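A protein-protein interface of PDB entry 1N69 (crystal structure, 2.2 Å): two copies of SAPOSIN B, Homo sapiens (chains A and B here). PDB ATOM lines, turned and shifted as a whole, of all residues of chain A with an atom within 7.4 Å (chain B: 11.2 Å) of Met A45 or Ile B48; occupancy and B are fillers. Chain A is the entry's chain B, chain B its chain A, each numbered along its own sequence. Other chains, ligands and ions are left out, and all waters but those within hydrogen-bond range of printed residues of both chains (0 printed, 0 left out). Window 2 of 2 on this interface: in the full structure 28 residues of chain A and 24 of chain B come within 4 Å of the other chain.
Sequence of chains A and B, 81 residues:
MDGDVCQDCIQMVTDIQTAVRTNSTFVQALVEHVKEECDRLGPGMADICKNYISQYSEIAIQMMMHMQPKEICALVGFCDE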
ATOM      1  N   CYS A  38      12.948 -14.065  -4.622  1.00  0.00           N
ATOM      2  CA  CYS A  38      12.919 -15.396  -4.042  1.00  0.00           C
ATOM      3  C   CYS A  38      11.507 -15.643  -3.505  1.00  0.00           C
ATOM      4  O   CYS A  38      11.064 -16.788  -3.391  1.00  0.00           O
ATOM      5  CB  CYS A  38      13.898 -15.492  -2.875  1.00  0.00           C
ATOM      6  SG  CYS A  38      15.653 -15.829  -3.231  1.00  0.00           S
ATOM      7  N   ASP A  39      10.814 -14.557  -3.169  1.00  0.00           N
ATOM      8  CA  ASP A  39       9.460 -14.637  -2.628  1.00  0.00           C
ATOM      9  C   ASP A  39       8.464 -15.257  -3.602  1.00  0.00           C
ATOM     10  O   ASP A  39       7.422 -15.758  -3.189  1.00  0.00           O
ATOM     11  CB  ASP A  39       8.954 -13.248  -2.213  1.00  0.00           C
ATOM     12  CG  ASP A  39       9.815 -12.605  -1.140  1.00  0.00           C
ATOM     13  OD1 ASP A  39      10.294 -13.328  -0.240  1.00  0.00           O
ATOM     14  OD2 ASP A  39      10.002 -11.370  -1.186  1.00  0.00           O
ATOM     15  N   ARG A  40       8.781 -15.225  -4.891  1.00  0.00           N
ATOM     16  CA  ARG A  40       7.891 -15.788  -5.898  1.00  0.00           C
ATOM     17  C   ARG A  40       7.822 -17.310  -5.798  1.00  0.00           C
ATOM     18  O   ARG A  40       6.966 -17.945  -6.417  1.00  0.00           O
ATOM     19  CB  ARG A  40       8.361 -15.386  -7.296  1.00  0.00           C
ATOM     20  CG  ARG A  40       8.690 -13.908  -7.430  1.00  0.00           C
ATOM     21  CD  ARG A  40       7.599 -13.037  -6.815  1.00  0.00           C
ATOM     22  NE  ARG A  40       7.805 -11.620  -7.101  1.00  0.00           N
ATOM     23  CZ  ARG A  40       6.984 -10.651  -6.711  1.00  0.00           C
ATOM     24  NH1 ARG A  40       5.896 -10.945  -6.013  1.00  0.00           N
ATOM     25  NH2 ARG A  40       7.244  -9.390  -7.029  1.00  0.00           N
ATOM     26  N   LEU A  41       8.730 -17.887  -5.016  1.00  0.00           N
ATOM     27  CA  LEU A  41       8.777 -19.334  -4.830  1.00  0.00           C
ATOM     28  C   LEU A  41       7.767 -19.759  -3.776  1.00  0.00           C
ATOM     29  O   LEU A  41       7.538 -20.952  -3.561  1.00  0.00           O
ATOM     30  CB  LEU A  41      10.182 -19.769  -4.399  1.00  0.00           C
ATOM     31  CG  LEU A  41      11.291 -19.549  -5.427  1.00  0.00           C
ATOM     32  CD1 LEU A  41      12.632 -19.957  -4.843  1.00  0.00           C
ATOM     33  CD2 LEU A  41      10.976 -20.352  -6.676  1.00  0.00           C
ATOM     34  N   GLY A  42       7.168 -18.768  -3.122  1.00  0.00           N
ATOM     35  CA  GLY A  42       6.185 -19.042  -2.093  1.00  0.00           C
ATOM     36  C   GLY A  42       6.826 -19.222  -0.732  1.00  0.00           C
ATOM     37  O   GLY A  42       8.044 -19.106  -0.596  1.00  0.00           O
ATOM     38  N   PRO A  43       6.023 -19.506   0.304  1.00  0.00           N
ATOM     39  CA  PRO A  43       6.543 -19.699   1.659  1.00  0.00           C
ATOM     40  C   PRO A  43       7.396 -20.960   1.762  1.00  0.00           C
ATOM     41  O   PRO A  43       7.063 -21.993   1.179  1.00  0.00           O
ATOM     42  CB  PRO A  43       5.275 -19.778   2.502  1.00  0.00           C
ATOM     43  CG  PRO A  43       4.299 -20.430   1.558  1.00  0.00           C
ATOM     44  CD  PRO A  43       4.561 -19.692   0.267  1.00  0.00           C
ATOM     45  N   GLY A  44       8.497 -20.869   2.500  1.00  0.00           N
ATOM     46  CA  GLY A  44       9.373 -22.014   2.657  1.00  0.00           C
ATOM     47  C   GLY A  44      10.582 -21.939   1.744  1.00  0.00           C
ATOM     48  O   GLY A  44      11.712 -21.778   2.208  1.00  0.00           O
ATOM     49  N   MET A  45      10.344 -22.051   0.441  1.00  0.00           N
ATOM     50  CA  MET A  45      11.425 -21.996  -0.536  1.00  0.00           C
ATOM     51  C   MET A  45      12.065 -20.615  -0.563  1.00  0.00           C
ATOM     52  O   MET A  45      13.279 -20.490  -0.718  1.00  0.00           O
ATOM     53  CB  MET A  45      10.895 -22.346  -1.927  1.00  0.00           C
ATOM     54  CG  MET A  45      10.172 -23.677  -1.981  1.00  0.00           C
ATOM     55  SD  MET A  45      11.193 -25.051  -1.419  1.00  0.00           S
ATOM     56  CE  MET A  45      11.781 -25.659  -2.987  1.00  0.00           C
ATOM     57  N   ALA A  46      11.242 -19.582  -0.411  1.00  0.00           N
ATOM     58  CA  ALA A  46      11.724 -18.207  -0.416  1.00  0.00           C
ATOM     59  C   ALA A  46      12.891 -18.056   0.549  1.00  0.00           C
ATOM     60  O   ALA A  46      13.823 -17.288   0.303  1.00  0.00           O
ATOM     61  CB  ALA A  46      10.600 -17.258  -0.026  1.00  0.00           C
ATOM     62  N   ASP A  47      12.834 -18.807   1.642  1.00  0.00           N
ATOM     63  CA  ASP A  47      13.871 -18.769   2.665  1.00  0.00           C
ATOM     64  C   ASP A  47      15.117 -19.551   2.262  1.00  0.00           C
ATOM     65  O   ASP A  47      16.233 -19.158   2.599  1.00  0.00           O
ATOM     66  CB  ASP A  47      13.307 -19.312   3.976  1.00  0.00           C
ATOM     67  CG  ASP A  47      12.085 -18.542   4.439  1.00  0.00           C
ATOM     68  OD1 ASP A  47      12.233 -17.347   4.782  1.00  0.00           O
ATOM     69  OD2 ASP A  47      10.980 -19.130   4.450  1.00  0.00           O
ATOM     70  N   ILE A  48      14.923 -20.657   1.546  1.00  0.00           N
ATOM     71  CA  ILE A  48      16.038 -21.485   1.082  1.00  0.00           C
ATOM     72  C   ILE A  48      16.827 -20.711   0.024  1.00  0.00           C
ATOM     73  O   ILE A  48      18.058 -20.732  -0.006  1.00  0.00           O
ATOM     74  CB  ILE A  48      15.529 -22.811   0.449  1.00  0.00           C
ATOM     75  CG1 ILE A  48      14.860 -23.683   1.515  1.00  0.00           C
ATOM     76  CG2 ILE A  48      16.684 -23.568  -0.195  1.00  0.00           C
ATOM     77  CD1 ILE A  48      14.366 -25.026   0.989  1.00  0.00           C
ATOM     78  N   CYS A  49      16.083 -20.026  -0.834  1.00  0.00           N
ATOM     79  CA  CYS A  49      16.612 -19.218  -1.925  1.00  0.00           C
ATOM     80  C   CYS A  49      17.391 -18.000  -1.404  1.00  0.00           C
ATOM     81  O   CYS A  49      18.559 -17.808  -1.757  1.00  0.00           O
ATOM     82  CB  CYS A  49      15.421 -18.810  -2.796  1.00  0.00           C
ATOM     83  SG  CYS A  49      15.611 -17.629  -4.171  1.00  0.00           S
ATOM     84  N   LYS A  50      16.756 -17.196  -0.552  1.00  0.00           N
ATOM     85  CA  LYS A  50      17.399 -16.007   0.013  1.00  0.00           C
ATOM     86  C   LYS A  50      18.718 -16.328   0.706  1.00  0.00           C
ATOM     87  O   LYS A  50      19.696 -15.595   0.568  1.00  0.00           O
ATOM     88  CB  LYS A  50      16.481 -15.315   1.025  1.00  0.00           C
ATOM     89  CG  LYS A  50      15.319 -14.544   0.434  1.00  0.00           C
ATOM     90  CD  LYS A  50      14.526 -13.845   1.535  1.00  0.00           C
ATOM     91  CE  LYS A  50      13.379 -13.021   0.969  1.00  0.00           C
ATOM     92  NZ  LYS A  50      13.869 -11.897   0.117  1.00  0.00           N
ATOM     93  N   ASN A  51      18.728 -17.417   1.464  1.00  0.00           N
ATOM     94  CA  ASN A  51      19.916 -17.840   2.199  1.00  0.00           C
ATOM     95  C   ASN A  51      20.997 -18.354   1.245  1.00  0.00           C
ATOM     96  O   ASN A  51      22.190 -18.162   1.481  1.00  0.00           O
ATOM     97  CB  ASN A  51      19.542 -18.947   3.191  1.00  0.00           C
ATOM     98  CG  ASN A  51      20.629 -19.210   4.214  1.00  0.00           C
ATOM     99  OD1 ASN A  51      20.807 -20.342   4.665  1.00  0.00           O
ATOM    100  ND2 ASN A  51      21.352 -18.162   4.597  1.00  0.00           N
ATOM    101  N   VAL B  31      14.202 -19.302 -21.140  1.00  0.00           N
ATOM    102  CA  VAL B  31      13.884 -19.941 -19.871  1.00  0.00           C
ATOM    103  C   VAL B  31      14.385 -21.389 -19.890  1.00  0.00           C
ATOM    104  O   VAL B  31      14.978 -21.863 -18.919  1.00  0.00           O
ATOM    105  CB  VAL B  31      12.366 -19.923 -19.612  1.00  0.00           C
ATOM    106  CG1 VAL B  31      12.035 -20.749 -18.355  1.00  0.00           C
ATOM    107  CG2 VAL B  31      11.891 -18.484 -19.443  1.00  0.00           C
ATOM    108  N   VAL B  34      18.163 -21.464 -19.405  1.00  0.00           N
ATOM    109  CA  VAL B  34      18.581 -21.157 -18.046  1.00  0.00           C
ATOM    110  C   VAL B  34      18.269 -22.305 -17.100  1.00  0.00           C
ATOM    111  O   VAL B  34      19.060 -22.606 -16.207  1.00  0.00           O
ATOM    112  CB  VAL B  34      17.919 -19.857 -17.534  1.00  0.00           C
ATOM    113  CG1 VAL B  34      18.232 -19.658 -16.057  1.00  0.00           C
ATOM    114  CG2 VAL B  34      18.434 -18.668 -18.343  1.00  0.00           C
ATOM    115  N   LYS B  35      17.123 -22.952 -17.302  1.00  0.00           N
ATOM    116  CA  LYS B  35      16.734 -24.079 -16.459  1.00  0.00           C
ATOM    117  C   LYS B  35      17.743 -25.199 -16.581  1.00  0.00           C
ATOM    118  O   LYS B  35      17.994 -25.919 -15.622  1.00  0.00           O
ATOM    119  CB  LYS B  35      15.352 -24.594 -16.839  1.00  0.00           C
ATOM    120  CG  LYS B  35      14.215 -23.778 -16.265  1.00  0.00           C
ATOM    121  CD  LYS B  35      12.900 -24.411 -16.658  1.00  0.00           C
ATOM    122  CE  LYS B  35      11.716 -23.680 -16.068  1.00  0.00           C
ATOM    123  NZ  LYS B  35      10.466 -24.341 -16.535  1.00  0.00           N
ATOM    124  N   GLU B  36      18.321 -25.342 -17.766  1.00  0.00           N
ATOM    125  CA  GLU B  36      19.333 -26.363 -18.006  1.00  0.00           C
ATOM    126  C   GLU B  36      20.620 -26.055 -17.237  1.00  0.00           C
ATOM    127  O   GLU B  36      21.297 -26.968 -16.754  1.00  0.00           O
ATOM    128  CB  GLU B  36      19.631 -26.466 -19.509  1.00  0.00           C
ATOM    129  CG  GLU B  36      20.930 -27.185 -19.834  1.00  0.00           C
ATOM    130  CD  GLU B  36      21.090 -27.487 -21.317  1.00  0.00           C
ATOM    131  OE1 GLU B  36      21.014 -26.542 -22.136  1.00  0.00           O
ATOM    132  OE2 GLU B  36      21.300 -28.674 -21.661  1.00  0.00           O
ATOM    133  N   GLU B  37      20.954 -24.771 -17.124  1.00  0.00           N
ATOM    134  CA  GLU B  37      22.160 -24.350 -16.404  1.00  0.00           C
ATOM    135  C   GLU B  37      21.953 -24.553 -14.912  1.00  0.00           C
ATOM    136  O   GLU B  37      22.909 -24.695 -14.148  1.00  0.00           O
ATOM    137  CB  GLU B  37      22.461 -22.873 -16.679  1.00  0.00           C
ATOM    138  CG  GLU B  37      22.616 -22.528 -18.156  1.00  0.00           C
ATOM    139  CD  GLU B  37      23.652 -23.391 -18.852  1.00  0.00           C
ATOM    140  OE1 GLU B  37      24.691 -23.697 -18.227  1.00  0.00           O
ATOM    141  OE2 GLU B  37      23.432 -23.759 -20.027  1.00  0.00           O
ATOM    142  N   CYS B  38      20.690 -24.554 -14.503  1.00  0.00           N
ATOM    143  CA  CYS B  38      20.332 -24.763 -13.110  1.00  0.00           C
ATOM    144  C   CYS B  38      20.856 -26.114 -12.617  1.00  0.00           C
ATOM    145  O   CYS B  38      21.124 -26.280 -11.426  1.00  0.00           O
ATOM    146  CB  CYS B  38      18.812 -24.733 -12.947  1.00  0.00           C
ATOM    147  SG  CYS B  38      18.002 -23.105 -12.724  1.00  0.00           S
ATOM    148  N   ASP B  39      20.985 -27.085 -13.526  1.00  0.00           N
ATOM    149  CA  ASP B  39      21.480 -28.409 -13.140  1.00  0.00           C
ATOM    150  C   ASP B  39      22.853 -28.338 -12.497  1.00  0.00           C
ATOM    151  O   ASP B  39      23.236 -29.240 -11.746  1.00  0.00           O
ATOM    152  CB  ASP B  39      21.539 -29.357 -14.341  1.00  0.00           C
ATOM    153  CG  ASP B  39      20.171 -29.764 -14.819  1.00  0.00           C
ATOM    154  OD1 ASP B  39      19.215 -29.682 -14.023  1.00  0.00           O
ATOM    155  OD2 ASP B  39      20.051 -30.175 -15.984  1.00  0.00           O
ATOM    156  N   ARG B  40      23.590 -27.272 -12.798  1.00  0.00           N
ATOM    157  CA  ARG B  40      24.916 -27.071 -12.225  1.00  0.00           C
ATOM    158  C   ARG B  40      24.859 -27.060 -10.696  1.00  0.00           C
ATOM    159  O   ARG B  40      25.855 -27.359 -10.028  1.00  0.00           O
ATOM    160  CB  ARG B  40      25.521 -25.752 -12.726  1.00  0.00           C
ATOM    161  CG  ARG B  40      25.943 -25.782 -14.195  1.00  0.00           C
ATOM    162  CD  ARG B  40      26.291 -24.390 -14.728  1.00  0.00           C
ATOM    163  NE  ARG B  40      26.456 -24.403 -16.183  1.00  0.00           N
ATOM    164  CZ  ARG B  40      27.565 -24.777 -16.815  1.00  0.00           C
ATOM    165  NH1 ARG B  40      28.626 -25.161 -16.129  1.00  0.00           N
ATOM    166  NH2 ARG B  40      27.600 -24.805 -18.140  1.00  0.00           N
ATOM    167  N   LEU B  41      23.693 -26.721 -10.146  1.00  0.00           N
ATOM    168  CA  LEU B  41      23.523 -26.679  -8.698  1.00  0.00           C
ATOM    169  C   LEU B  41      23.384 -28.056  -8.043  1.00  0.00           C
ATOM    170  O   LEU B  41      23.384 -28.158  -6.819  1.00  0.00           O
ATOM    171  CB  LEU B  41      22.313 -25.817  -8.330  1.00  0.00           C
ATOM    172  CG  LEU B  41      22.384 -24.355  -8.775  1.00  0.00           C
ATOM    173  CD1 LEU B  41      21.257 -23.576  -8.109  1.00  0.00           C
ATOM    174  CD2 LEU B  41      23.729 -23.756  -8.392  1.00  0.00           C
ATOM    175  N   GLY B  42      23.254 -29.103  -8.859  1.00  0.00           N
ATOM    176  CA  GLY B  42      23.138 -30.451  -8.334  1.00  0.00           C
ATOM    177  C   GLY B  42      21.775 -30.808  -7.777  1.00  0.00           C
ATOM    178  O   GLY B  42      20.912 -29.940  -7.644  1.00  0.00           O
ATOM    179  N   PRO B  43      21.552 -32.091  -7.442  1.00  0.00           N
ATOM    180  CA  PRO B  43      20.287 -32.592  -6.887  1.00  0.00           C
ATOM    181  C   PRO B  43      19.766 -31.785  -5.701  1.00  0.00           C
ATOM    182  O   PRO B  43      20.513 -31.411  -4.795  1.00  0.00           O
ATOM    183  CB  PRO B  43      20.603 -34.055  -6.525  1.00  0.00           C
ATOM    184  CG  PRO B  43      22.104 -34.145  -6.554  1.00  0.00           C
ATOM    185  CD  PRO B  43      22.507 -33.195  -7.637  1.00  0.00           C
ATOM    186  N   GLY B  44      18.469 -31.518  -5.728  1.00  0.00           N
ATOM    187  CA  GLY B  44      17.852 -30.738  -4.678  1.00  0.00           C
ATOM    188  C   GLY B  44      17.772 -29.285  -5.102  1.00  0.00           C
ATOM    189  O   GLY B  44      16.718 -28.816  -5.523  1.00  0.00           O
ATOM    190  N   MET B  45      18.897 -28.582  -5.018  1.00  0.00           N
ATOM    191  CA  MET B  45      18.952 -27.167  -5.376  1.00  0.00           C
ATOM    192  C   MET B  45      18.666 -26.842  -6.841  1.00  0.00           C
ATOM    193  O   MET B  45      18.120 -25.783  -7.141  1.00  0.00           O
ATOM    194  CB  MET B  45      20.313 -26.583  -4.977  1.00  0.00           C
ATOM    195  CG  MET B  45      20.600 -26.663  -3.470  1.00  0.00           C
ATOM    196  SD  MET B  45      19.362 -25.795  -2.460  1.00  0.00           S
ATOM    197  CE  MET B  45      18.335 -27.148  -1.937  1.00  0.00           C
ATOM    198  N   ALA B  46      19.035 -27.741  -7.750  1.00  0.00           N
ATOM    199  CA  ALA B  46      18.800 -27.520  -9.173  1.00  0.00           C
ATOM    200  C   ALA B  46      17.330 -27.247  -9.493  1.00  0.00           C
ATOM    201  O   ALA B  46      17.011 -26.261 -10.154  1.00  0.00           O
ATOM    202  CB  ALA B  46      19.289 -28.720  -9.987  1.00  0.00           C
ATOM    203  N   ASP B  47      16.437 -28.119  -9.028  1.00  0.00           N
ATOM    204  CA  ASP B  47      15.014 -27.952  -9.301  1.00  0.00           C
ATOM    205  C   ASP B  47      14.396 -26.713  -8.658  1.00  0.00           C
ATOM    206  O   ASP B  47      13.385 -26.207  -9.132  1.00  0.00           O
ATOM    207  CB  ASP B  47      14.241 -29.208  -8.889  1.00  0.00           C
ATOM    208  CG  ASP B  47      14.428 -30.359  -9.880  1.00  0.00           C
ATOM    209  OD1 ASP B  47      15.142 -30.176 -10.892  1.00  0.00           O
ATOM    210  OD2 ASP B  47      13.855 -31.443  -9.647  1.00  0.00           O
ATOM    211  N   ILE B  48      14.989 -26.223  -7.580  1.00  0.00           N
ATOM    212  CA  ILE B  48      14.458 -25.016  -6.952  1.00  0.00           C
ATOM    213  C   ILE B  48      14.805 -23.851  -7.884  1.00  0.00           C
ATOM    214  O   ILE B  48      13.985 -22.968  -8.146  1.00  0.00           O
ATOM    215  CB  ILE B  48      15.094 -24.762  -5.571  1.00  0.00           C
ATOM    216  CG1 ILE B  48      14.770 -25.923  -4.630  1.00  0.00           C
ATOM    217  CG2 ILE B  48      14.571 -23.457  -4.994  1.00  0.00           C
ATOM    218  CD1 ILE B  48      15.439 -25.813  -3.267  1.00  0.00           C
ATOM    219  N   CYS B  49      16.037 -23.876  -8.380  1.00  0.00           N
ATOM    220  CA  CYS B  49      16.549 -22.869  -9.300  1.00  0.00           C
ATOM    221  C   CYS B  49      15.654 -22.827 -10.535  1.00  0.00           C
ATOM    222  O   CYS B  49      15.352 -21.750 -11.065  1.00  0.00           O
ATOM    223  CB  CYS B  49      17.982 -23.246  -9.677  1.00  0.00           C
ATOM    224  SG  CYS B  49      18.840 -22.362 -11.026  1.00  0.00           S
ATOM    225  N   LYS B  50      15.218 -24.003 -10.983  1.00  0.00           N
ATOM    226  CA  LYS B  50      14.358 -24.080 -12.156  1.00  0.00           C
ATOM    227  C   LYS B  50      13.028 -23.398 -11.891  1.00  0.00           C
ATOM    228  O   LYS B  50      12.535 -22.652 -12.740  1.00  0.00           O
ATOM    229  CB  LYS B  50      14.153 -25.538 -12.577  1.00  0.00           C
ATOM    230  CG  LYS B  50      15.438 -26.167 -13.094  1.00  0.00           C
ATOM    231  CD  LYS B  50      15.248 -27.560 -13.662  1.00  0.00           C
ATOM    232  CE  LYS B  50      16.576 -28.081 -14.196  1.00  0.00           C
ATOM    233  NZ  LYS B  50      16.432 -29.272 -15.057  1.00  0.00           N
ATOM    234  N   ASN B  51      12.450 -23.645 -10.717  1.00  0.00           N
ATOM    235  CA  ASN B  51      11.185 -23.017 -10.354  1.00  0.00           C
ATOM    236  C   ASN B  51      11.395 -21.510 -10.276  1.00  0.00           C
ATOM    237  O   ASN B  51      10.582 -20.740 -10.776  1.00  0.00           O
ATOM    238  CB  ASN B  51      10.681 -23.526  -9.001  1.00  0.00           C
ATOM    239  CG  ASN B  51      10.442 -25.021  -8.990  1.00  0.00           C
ATOM    240  OD1 ASN B  51       9.932 -25.590  -9.960  1.00  0.00           O
ATOM    241  ND2 ASN B  51      10.797 -25.667  -7.881  1.00  0.00           N
ATOM    242  N   TYR B  52      12.499 -21.105  -9.650  1.00  0.00           N
ATOM    243  CA  TYR B  52      12.850 -19.694  -9.504  1.00  0.00           C
ATOM    244  C   TYR B  52      12.867 -18.984 -10.855  1.00  0.00           C
ATOM    245  O   TYR B  52      12.316 -17.891 -11.007  1.00  0.00           O
ATOM    246  CB  TYR B  52      14.238 -19.549  -8.862  1.00  0.00           C
ATOM    247  CG  TYR B  52      14.679 -18.111  -8.719  1.00  0.00           C
ATOM    248  CD1 TYR B  52      14.345 -17.366  -7.585  1.00  0.00           C
ATOM    249  CD2 TYR B  52      15.368 -17.468  -9.749  1.00  0.00           C
ATOM    250  CE1 TYR B  52      14.684 -16.015  -7.482  1.00  0.00           C
ATOM    251  CE2 TYR B  52      15.707 -16.119  -9.661  1.00  0.00           C
ATOM    252  CZ  TYR B  52      15.362 -15.397  -8.528  1.00  0.00           C
ATOM    253  OH  TYR B  52      15.681 -14.058  -8.450  1.00  0.00           O
ATOM    254  N   ILE B  53      13.525 -19.609 -11.826  1.00  0.00           N
ATOM    255  CA  ILE B  53      13.642 -19.057 -13.167  1.00  0.00           C
ATOM    256  C   ILE B  53      12.279 -18.967 -13.816  1.00  0.00           C
ATOM    257  O   ILE B  53      11.972 -18.008 -14.521  1.00  0.00           O
ATOM    258  CB  ILE B  53      14.548 -19.941 -14.054  1.00  0.00           C
ATOM    259  CG1 ILE B  53      15.965 -19.986 -13.466  1.00  0.00           C
ATOM    260  CG2 ILE B  53      14.557 -19.411 -15.483  1.00  0.00           C
ATOM    261  CD1 ILE B  53      16.624 -18.616 -13.321  1.00  0.00           C
ATOM    262  N   SER B  54      11.465 -19.987 -13.579  1.00  0.00           N
ATOM    263  CA  SER B  54      10.126 -20.040 -14.135  1.00  0.00           C
ATOM    264  C   SER B  54       9.322 -18.867 -13.581  1.00  0.00           C
ATOM    265  O   SER B  54       8.621 -18.173 -14.315  1.00  0.00           O
ATOM    266  CB  SER B  54       9.472 -21.367 -13.752  1.00  0.00           C
ATOM    267  OG  SER B  54       8.173 -21.471 -14.291  1.00  0.00           O
ATOM    268  N   GLN B  55       9.446 -18.644 -12.278  1.00  0.00           N
ATOM    269  CA  GLN B  55       8.736 -17.562 -11.621  1.00  0.00           C
ATOM    270  C   GLN B  55       9.274 -16.191 -12.006  1.00  0.00           C
ATOM    271  O   GLN B  55       8.506 -15.263 -12.244  1.00  0.00           O
ATOM    272  CB  GLN B  55       8.821 -17.735 -10.107  1.00  0.00           C
ATOM    273  CG  GLN B  55       8.162 -19.010  -9.602  1.00  0.00           C
ATOM    274  CD  GLN B  55       6.673 -19.040  -9.880  1.00  0.00           C
ATOM    275  OE1 GLN B  55       5.916 -18.229  -9.346  1.00  0.00           O
ATOM    276  NE2 GLN B  55       6.244 -19.974 -10.724  1.00  0.00           N
ATOM    277  N   TYR B  56      10.595 -16.063 -12.073  1.00  0.00           N
ATOM    278  CA  TYR B  56      11.207 -14.786 -12.413  1.00  0.00           C
ATOM    279  C   TYR B  56      10.872 -14.309 -13.822  1.00  0.00           C
ATOM    280  O   TYR B  56      10.662 -13.118 -14.044  1.00  0.00           O
ATOM    281  CB  TYR B  56      12.729 -14.858 -12.260  1.00  0.00           C
ATOM    282  CG  TYR B  56      13.396 -13.515 -12.450  1.00  0.00           C
ATOM    283  CD1 TYR B  56      13.402 -12.566 -11.426  1.00  0.00           C
ATOM    284  CD2 TYR B  56      13.966 -13.164 -13.675  1.00  0.00           C
ATOM    285  CE1 TYR B  56      13.954 -11.302 -11.612  1.00  0.00           C
ATOM    286  CE2 TYR B  56      14.522 -11.902 -13.874  1.00  0.00           C
ATOM    287  CZ  TYR B  56      14.512 -10.976 -12.839  1.00  0.00           C
ATOM    288  OH  TYR B  56      15.053  -9.723 -13.032  1.00  0.00           O
ATOM    289  N   SER B  57      10.829 -15.237 -14.772  1.00  0.00           N
ATOM    290  CA  SER B  57      10.534 -14.896 -16.156  1.00  0.00           C
ATOM    291  C   SER B  57       9.132 -14.314 -16.306  1.00  0.00           C
ATOM    292  O   SER B  57       8.922 -13.377 -17.082  1.00  0.00           O
ATOM    293  CB  SER B  57      10.694 -16.130 -17.055  1.00  0.00           C
ATOM    294  OG  SER B  57       9.920 -17.221 -16.583  1.00  0.00           O
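OE1 of Gln B55 lies close to O of Arg A40.
The side-chain sulfur (SG) of Cys A38 is in hydrogen-bond range of the backbone NH (N) of Lys A50 (3.2 Å). The side-chain sulfur (SG) of Cys A38 is disulfide-bonded to the side-chain sulfur (SG) of Cys A49, at 2.0 Å. The side-chain sulfur (SG) of Cys B49 is disulfide-bonded to the side-chain sulfur (SG) of Cys B38, at 2.0 Å. O of Asp B47 is in hydrogen-bond range of ND2 of Asn B51, at 2.9 Å.
Cys A38 touches Tyr B52 (N to CE1, 3.9 Å). Leu A41 touches Asn B51 (CD2 to C, 3.8 Å). CD2 of Leu A41 touches N of Tyr B52 (3.4 Å). CE of Met A45 touches CG1 of Ile B48, 3.4 Å away. Cys A49 touches Tyr B52 (SG to CD1, 3.7 Å).
Of the printed residues of chain B, Arg A40 touches Gln B55. No residue of chain B comes within 4 Å of Pro A43. Of chain B, only Ile B48 (3.4 Å) comes within 4 Å of Met A45. Ala A46 touches none of the printed residues of chain B. No residue of chain B comes within 4 Å of Asp A47. Gly B42 touches none of the printed residues of chain A. Printed residues of chain A within 4 Å of Ile B48: Met A45. Lys B50 touches none of the printed residues of chain A. Of the printed residues of chain A, Tyr B52 touches Cys A38, Leu A41 and Cys A49. Printed residues of chain A within 4 Å of Gln B55: Arg A40. The nearest residue of chain B that does not touch Met A45 is Asn B51 (5.0 Å). The nearest printed residue of chain A that does not touch Ile B48 is Ile A48 (4.003 Å). The nearest printed residue of chain B that does not touch Arg A40 is Tyr B56 (5.3 Å).
Of the 25 printed residues of chain B, 4 touch a printed residue of chain A. Printed residues of chain B that touch a printed residue of chain A: Ile B48, Asn B51, Tyr B52 and Gln B55. Of the 14 printed residues of chain A, 5 touch a printed residue of chain B. Printed residues of chain A that touch a printed residue of chain B: Cys A38, Arg A40, Leu A41, Met A45 and Cys A49. Hydrophobic or aromatic side chains of chain A within 4 Å of the printed part of chain B: Leu A41 and Met A45. Among the printed residues, no Asp or Glu carboxylate lies within 4 Å of a Lys or Arg side-chain nitrogen of the other chain.
Leu A41 touches Asn B51, but with the chains exchanged Asn A51 does not touch Leu B41 (10.7 Å). Met A45 touches Ile B48, but with the chains exchanged Ile A48 does not touch Met B45 (4.2 Å). Positions printed for both chains: 38, 39, 40, 41, 42, 43, 44, 45, 46, 47, 48, 49, 50 and 51.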
